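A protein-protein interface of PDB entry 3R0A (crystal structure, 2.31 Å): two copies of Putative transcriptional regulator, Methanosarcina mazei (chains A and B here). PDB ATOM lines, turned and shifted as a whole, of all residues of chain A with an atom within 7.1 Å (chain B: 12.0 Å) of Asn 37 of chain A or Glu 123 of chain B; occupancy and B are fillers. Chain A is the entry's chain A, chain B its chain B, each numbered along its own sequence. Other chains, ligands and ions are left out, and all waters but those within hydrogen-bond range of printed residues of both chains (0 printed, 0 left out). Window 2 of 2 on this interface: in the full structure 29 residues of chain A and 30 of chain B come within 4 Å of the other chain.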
ATOM      1  N   SER A   1      26.190  25.188  15.449  1.00  0.00           N
ATOM      2  CA  SER A   1      25.354  26.304  15.993  1.00  0.00           C
ATOM      3  C   SER A   1      26.282  27.391  16.546  1.00  0.00           C
ATOM      4  O   SER A   1      26.296  27.648  17.767  1.00  0.00           O
ATOM      5  CB  SER A   1      24.387  25.764  17.063  1.00  0.00           C
ATOM      6  OG  SER A   1      24.986  24.716  17.827  1.00  0.00           O
ATOM      7  N   MET A  32      16.639  25.926   5.508  1.00  0.00           N
ATOM      8  CA  MET A  32      16.577  24.630   6.198  1.00  0.00           C
ATOM      9  C   MET A  32      16.322  24.803   7.698  1.00  0.00           C
ATOM     10  O   MET A  32      15.530  24.084   8.265  1.00  0.00           O
ATOM     11  CB  MET A  32      17.861  23.819   5.988  1.00  0.00           C
ATOM     12  CG  MET A  32      17.768  22.383   6.515  1.00  0.00           C
ATOM     13  SD  MET A  32      19.390  21.346   6.107  1.00  0.00           S
ATOM     14  CE  MET A  32      20.509  22.462   7.102  1.00  0.00           C
ATOM     15  N   LYS A  33      17.013  25.757   8.319  1.00  0.00           N
ATOM     16  CA  LYS A  33      16.838  26.053   9.751  1.00  0.00           C
ATOM     17  C   LYS A  33      15.360  26.333  10.123  1.00  0.00           C
ATOM     18  O   LYS A  33      14.843  25.734  11.072  1.00  0.00           O
ATOM     19  CB  LYS A  33      17.812  27.158  10.214  1.00  0.00           C
ATOM     20  CG  LYS A  33      19.271  26.613  10.421  1.00  0.00           C
ATOM     21  CD  LYS A  33      20.203  27.535  11.245  1.00  0.00           C
ATOM     22  CE  LYS A  33      21.018  28.470  10.383  1.00  0.00           C
ATOM     23  NZ  LYS A  33      22.097  29.129  11.190  1.00  0.00           N
ATOM     24  N   SER A  34      14.668  27.148   9.320  1.00  0.00           N
ATOM     25  CA  SER A  34      13.250  27.473   9.566  1.00  0.00           C
ATOM     26  C   SER A  34      12.386  26.225   9.638  1.00  0.00           C
ATOM     27  O   SER A  34      11.430  26.141  10.428  1.00  0.00           O
ATOM     28  CB  SER A  34      12.712  28.377   8.471  1.00  0.00           C
ATOM     29  OG  SER A  34      13.601  29.447   8.240  1.00  0.00           O
ATOM     30  N   PHE A  35      12.721  25.254   8.796  1.00  0.00           N
ATOM     31  CA  PHE A  35      11.965  24.030   8.753  1.00  0.00           C
ATOM     32  C   PHE A  35      12.261  23.157   9.959  1.00  0.00           C
ATOM     33  O   PHE A  35      11.383  22.440  10.435  1.00  0.00           O
ATOM     34  CB  PHE A  35      12.253  23.276   7.463  1.00  0.00           C
ATOM     35  CG  PHE A  35      11.490  23.788   6.281  1.00  0.00           C
ATOM     36  CD1 PHE A  35      12.088  24.643   5.377  1.00  0.00           C
ATOM     37  CD2 PHE A  35      10.175  23.412   6.067  1.00  0.00           C
ATOM     38  CE1 PHE A  35      11.384  25.128   4.283  1.00  0.00           C
ATOM     39  CE2 PHE A  35       9.476  23.897   4.967  1.00  0.00           C
ATOM     40  CZ  PHE A  35      10.094  24.751   4.076  1.00  0.00           C
ATOM     41  N   LEU A  36      13.503  23.228  10.446  1.00  0.00           N
ATOM     42  CA  LEU A  36      13.914  22.491  11.658  1.00  0.00           C
ATOM     43  C   LEU A  36      13.273  23.073  12.916  1.00  0.00           C
ATOM     44  O   LEU A  36      12.914  22.337  13.827  1.00  0.00           O
ATOM     45  CB  LEU A  36      15.439  22.483  11.793  1.00  0.00           C
ATOM     46  CG  LEU A  36      16.195  21.754  10.666  1.00  0.00           C
ATOM     47  CD1 LEU A  36      17.665  22.132  10.666  1.00  0.00           C
ATOM     48  CD2 LEU A  36      16.023  20.244  10.736  1.00  0.00           C
ATOM     49  N   ASN A  37      13.140  24.400  12.937  1.00  0.00           N
ATOM     50  CA  ASN A  37      12.405  25.112  13.983  1.00  0.00           C
ATOM     51  C   ASN A  37      10.916  24.724  14.016  1.00  0.00           C
ATOM     52  O   ASN A  37      10.304  24.687  15.092  1.00  0.00           O
ATOM     53  CB  ASN A  37      12.548  26.623  13.811  1.00  0.00           C
ATOM     54  CG  ASN A  37      13.984  27.097  13.905  1.00  0.00           C
ATOM     55  OD1 ASN A  37      14.236  28.273  14.170  1.00  0.00           O
ATOM     56  ND2 ASN A  37      14.940  26.192  13.695  1.00  0.00           N
ATOM     57  N   GLU A  38      10.343  24.410  12.850  1.00  0.00           N
ATOM     58  CA  GLU A  38       8.938  23.989  12.786  1.00  0.00           C
ATOM     59  C   GLU A  38       8.694  22.659  12.060  1.00  0.00           C
ATOM     60  O   GLU A  38       8.008  22.613  11.028  1.00  0.00           O
ATOM     61  CB  GLU A  38       8.069  25.122  12.229  1.00  0.00           C
ATOM     62  CG  GLU A  38       7.692  26.151  13.290  1.00  0.00           C
ATOM     63  CD  GLU A  38       7.060  27.400  12.709  1.00  0.00           C
ATOM     64  OE1 GLU A  38       7.751  28.437  12.637  1.00  0.00           O
ATOM     65  OE2 GLU A  38       5.871  27.350  12.322  1.00  0.00           O
ATOM     66  N   PRO A  39       9.195  21.550  12.645  1.00  0.00           N
ATOM     67  CA  PRO A  39       9.259  20.234  11.987  1.00  0.00           C
ATOM     68  C   PRO A  39       7.913  19.727  11.473  1.00  0.00           C
ATOM     69  O   PRO A  39       7.871  18.759  10.698  1.00  0.00           O
ATOM     70  CB  PRO A  39       9.767  19.318  13.096  1.00  0.00           C
ATOM     71  CG  PRO A  39       9.273  19.966  14.341  1.00  0.00           C
ATOM     72  CD  PRO A  39       9.417  21.436  14.099  1.00  0.00           C
ATOM     73  N   ASP A  40       6.830  20.380  11.901  1.00  0.00           N
ATOM     74  CA  ASP A  40       5.458  19.984  11.510  1.00  0.00           C
ATOM     75  C   ASP A  40       4.747  20.953  10.568  1.00  0.00           C
ATOM     76  O   ASP A  40       3.884  20.531   9.810  1.00  0.00           O
ATOM     77  CB  ASP A  40       4.590  19.753  12.734  1.00  0.00           C
ATOM     78  CG  ASP A  40       5.054  18.583  13.550  1.00  0.00           C
ATOM     79  OD1 ASP A  40       5.023  17.440  13.014  1.00  0.00           O
ATOM     80  OD2 ASP A  40       5.451  18.823  14.720  1.00  0.00           O
ATOM     81  N   ARG A  41       5.108  22.235  10.621  1.00  0.00           N
ATOM     82  CA  ARG A  41       4.549  23.226   9.705  1.00  0.00           C
ATOM     83  C   ARG A  41       4.788  22.842   8.226  1.00  0.00           C
ATOM     84  O   ARG A  41       5.897  22.445   7.831  1.00  0.00           O
ATOM     85  CB  ARG A  41       5.097  24.635  10.004  1.00  0.00           C
ATOM     86  CG  ARG A  41       4.399  25.804   9.220  1.00  0.00           C
ATOM     87  CD  ARG A  41       5.227  27.136   9.176  1.00  0.00           C
ATOM     88  NE  ARG A  41       6.631  26.971   8.736  1.00  0.00           N
ATOM     89  CZ  ARG A  41       7.496  27.964   8.470  1.00  0.00           C
ATOM     90  NH1 ARG A  41       7.144  29.246   8.571  1.00  0.00           N
ATOM     91  NH2 ARG A  41       8.735  27.677   8.094  1.00  0.00           N
ATOM     92  N   ILE A  90       9.634  19.668   6.608  1.00  0.00           N
ATOM     93  CA  ILE A  90      10.938  19.077   6.942  1.00  0.00           C
ATOM     94  C   ILE A  90      10.754  17.630   7.336  1.00  0.00           C
ATOM     95  O   ILE A  90       9.992  17.344   8.242  1.00  0.00           O
ATOM     96  CB  ILE A  90      11.639  19.853   8.096  1.00  0.00           C
ATOM     97  CG1 ILE A  90      13.085  20.216   7.733  1.00  0.00           C
ATOM     98  CG2 ILE A  90      11.516  19.124   9.468  1.00  0.00           C
ATOM     99  CD1 ILE A  90      14.019  19.060   7.521  1.00  0.00           C
ATOM    100  N   GLU B 114      28.376  15.208  17.505  1.00  0.00           N
ATOM    101  CA  GLU B 114      28.380  16.656  17.581  1.00  0.00           C
ATOM    102  C   GLU B 114      27.309  17.282  16.719  1.00  0.00           C
ATOM    103  O   GLU B 114      26.754  18.318  17.075  1.00  0.00           O
ATOM    104  CB  GLU B 114      29.746  17.219  17.239  1.00  0.00           C
ATOM    105  CG  GLU B 114      30.604  17.490  18.473  1.00  0.00           C
ATOM    106  CD  GLU B 114      30.511  18.941  18.984  1.00  0.00           C
ATOM    107  OE1 GLU B 114      29.477  19.624  18.784  1.00  0.00           O
ATOM    108  OE2 GLU B 114      31.504  19.415  19.586  1.00  0.00           O
ATOM    109  N   LEU B 115      26.996  16.647  15.603  1.00  0.00           N
ATOM    110  CA  LEU B 115      25.931  17.144  14.752  1.00  0.00           C
ATOM    111  C   LEU B 115      24.521  17.012  15.330  1.00  0.00           C
ATOM    112  O   LEU B 115      23.635  17.762  14.947  1.00  0.00           O
ATOM    113  CB  LEU B 115      26.008  16.525  13.365  1.00  0.00           C
ATOM    114  CG  LEU B 115      26.737  17.422  12.369  1.00  0.00           C
ATOM    115  CD1 LEU B 115      28.226  17.210  12.382  1.00  0.00           C
ATOM    116  CD2 LEU B 115      26.203  17.153  10.997  1.00  0.00           C
ATOM    117  N   LYS B 116      24.307  16.094  16.265  1.00  0.00           N
ATOM    118  CA  LYS B 116      22.963  15.931  16.821  1.00  0.00           C
ATOM    119  C   LYS B 116      22.740  16.749  18.103  1.00  0.00           C
ATOM    120  O   LYS B 116      21.614  16.845  18.605  1.00  0.00           O
ATOM    121  CB  LYS B 116      22.557  14.436  16.908  1.00  0.00           C
ATOM    122  CG  LYS B 116      22.753  13.693  18.218  1.00  0.00           C
ATOM    123  CD  LYS B 116      22.409  12.234  17.994  1.00  0.00           C
ATOM    124  CE  LYS B 116      21.411  11.711  19.016  1.00  0.00           C
ATOM    125  NZ  LYS B 116      22.000  11.289  20.317  1.00  0.00           N
ATOM    126  N   GLU B 117      23.826  17.334  18.616  1.00  0.00           N
ATOM    127  CA  GLU B 117      23.759  18.475  19.541  1.00  0.00           C
ATOM    128  C   GLU B 117      23.620  19.779  18.769  1.00  0.00           C
ATOM    129  O   GLU B 117      23.530  20.862  19.365  1.00  0.00           O
ATOM    130  CB  GLU B 117      25.016  18.570  20.394  1.00  0.00           C
ATOM    131  CG  GLU B 117      24.893  17.939  21.750  1.00  0.00           C
ATOM    132  CD  GLU B 117      26.105  17.113  22.058  1.00  0.00           C
ATOM    133  OE1 GLU B 117      27.174  17.717  22.312  1.00  0.00           O
ATOM    134  OE2 GLU B 117      25.990  15.862  22.022  1.00  0.00           O
ATOM    135  N   TRP B 118      23.642  19.681  17.445  1.00  0.00           N
ATOM    136  CA  TRP B 118      23.437  20.846  16.613  1.00  0.00           C
ATOM    137  C   TRP B 118      21.950  21.071  16.445  1.00  0.00           C
ATOM    138  O   TRP B 118      21.464  22.173  16.692  1.00  0.00           O
ATOM    139  CB  TRP B 118      24.116  20.709  15.258  1.00  0.00           C
ATOM    140  CG  TRP B 118      23.785  21.850  14.368  1.00  0.00           C
ATOM    141  CD1 TRP B 118      24.190  23.138  14.519  1.00  0.00           C
ATOM    142  CD2 TRP B 118      22.947  21.823  13.205  1.00  0.00           C
ATOM    143  NE1 TRP B 118      23.680  23.917  13.519  1.00  0.00           N
ATOM    144  CE2 TRP B 118      22.905  23.140  12.698  1.00  0.00           C
ATOM    145  CE3 TRP B 118      22.238  20.817  12.539  1.00  0.00           C
ATOM    146  CZ2 TRP B 118      22.177  23.484  11.544  1.00  0.00           C
ATOM    147  CZ3 TRP B 118      21.514  21.158  11.390  1.00  0.00           C
ATOM    148  CH2 TRP B 118      21.492  22.481  10.909  1.00  0.00           C
ATOM    149  N   GLU B 119      21.246  20.018  16.038  1.00  0.00           N
ATOM    150  CA  GLU B 119      19.796  20.045  15.877  1.00  0.00           C
ATOM    151  C   GLU B 119      19.096  20.284  17.231  1.00  0.00           C
ATOM    152  O   GLU B 119      18.405  21.298  17.410  1.00  0.00           O
ATOM    153  CB  GLU B 119      19.322  18.746  15.206  1.00  0.00           C
ATOM    154  CG  GLU B 119      18.357  18.946  14.025  1.00  0.00           C
ATOM    155  CD  GLU B 119      16.890  18.595  14.336  1.00  0.00           C
ATOM    156  OE1 GLU B 119      16.397  17.587  13.781  1.00  0.00           O
ATOM    157  OE2 GLU B 119      16.227  19.324  15.115  1.00  0.00           O
ATOM    158  N   ASN B 120      19.309  19.370  18.180  1.00  0.00           N
ATOM    159  CA  ASN B 120      18.787  19.506  19.555  1.00  0.00           C
ATOM    160  C   ASN B 120      19.588  20.494  20.445  1.00  0.00           C
ATOM    161  O   ASN B 120      20.284  20.094  21.395  1.00  0.00           O
ATOM    162  CB  ASN B 120      18.688  18.125  20.222  1.00  0.00           C
ATOM    163  CG  ASN B 120      18.060  18.186  21.608  1.00  0.00           C
ATOM    164  OD1 ASN B 120      16.849  18.420  21.757  1.00  0.00           O
ATOM    165  ND2 ASN B 120      18.887  17.983  22.633  1.00  0.00           N
ATOM    166  N   GLY B 121      19.459  21.782  20.129  1.00  0.00           N
ATOM    167  CA  GLY B 121      20.265  22.853  20.737  1.00  0.00           C
ATOM    168  C   GLY B 121      20.387  24.031  19.775  1.00  0.00           C
ATOM    169  O   GLY B 121      20.846  25.122  20.151  1.00  0.00           O
ATOM    170  N   GLY B 122      19.972  23.795  18.528  1.00  0.00           N
ATOM    171  CA  GLY B 122      19.938  24.817  17.481  1.00  0.00           C
ATOM    172  C   GLY B 122      18.719  25.714  17.592  1.00  0.00           C
ATOM    173  O   GLY B 122      18.696  26.802  17.002  1.00  0.00           O
ATOM    174  N   GLU B 123      17.707  25.254  18.340  1.00  0.00           N
ATOM    175  CA  GLU B 123      16.516  26.057  18.681  1.00  0.00           C
ATOM    176  C   GLU B 123      15.645  26.378  17.455  1.00  0.00           C
ATOM    177  O   GLU B 123      14.412  26.321  17.514  1.00  0.00           O
ATOM    178  CB  GLU B 123      16.928  27.329  19.464  1.00  0.00           C
ATOM    179  CG  GLU B 123      15.881  28.454  19.581  1.00  0.00           C
ATOM    180  CD  GLU B 123      16.124  29.597  18.600  1.00  0.00           C
ATOM    181  OE1 GLU B 123      16.415  30.719  19.063  1.00  0.00           O
ATOM    182  OE2 GLU B 123      16.030  29.375  17.373  1.00  0.00           O
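N of Ser 1 of chain A lies close to NE1 of Trp 118 of chain B (3.4 Å).
O of Lys 33 of chain A is in hydrogen-bond range of ND2 of Asn 37 of chain A (2.7 Å).
Among the printed residues, pairs that only touch across the chains: Asn 37 of chain A with Glu 123 of chain B, Leu 36 of chain A with Trp 118 of chain B and Met 32 of chain A with Trp 118 of chain B.
Printed residues of chain B within 4 Å of Met 32 of chain A: Trp 118. Leu 36 of chain A touches just one residue of chain B: Trp 118 (3.9 Å). Asn 37 of chain A touches just one residue of chain B: Glu 123 (3.7 Å). No residue of chain B comes within 4 Å of Glu 38 of chain A. Pro 39 of chain A touches none of the printed residues of chain B. Of the printed residues of chain A, Trp 118 of chain B touches Ser 1 (3.0 Å), Met 32 (3.9 Å) and Leu 36 (3.9 Å). No residue of chain A comes within 4 Å of Gly 122 of chain B. The nearest residue of chain B that does not touch Asn 37 of chain A is Gly 122 of chain B (5.0 Å).
Of the 12 printed residues of chain A, 4 touch a printed residue of chain B. Printed residues of chain A that touch a printed residue of chain B: Ser 1, Met 32, Leu 36 and Asn 37. Hydrophobic or aromatic side chains of chain A within 4 Å of the printed part of chain B: Met 32 and Leu 36. Of the 10 printed residues of chain B, 2 touch a printed residue of chain A.
No position is printed for both chains. Of the 4 pairs that touch across the chains among the printed residues, none has its exchanged pair printed and touching as well.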
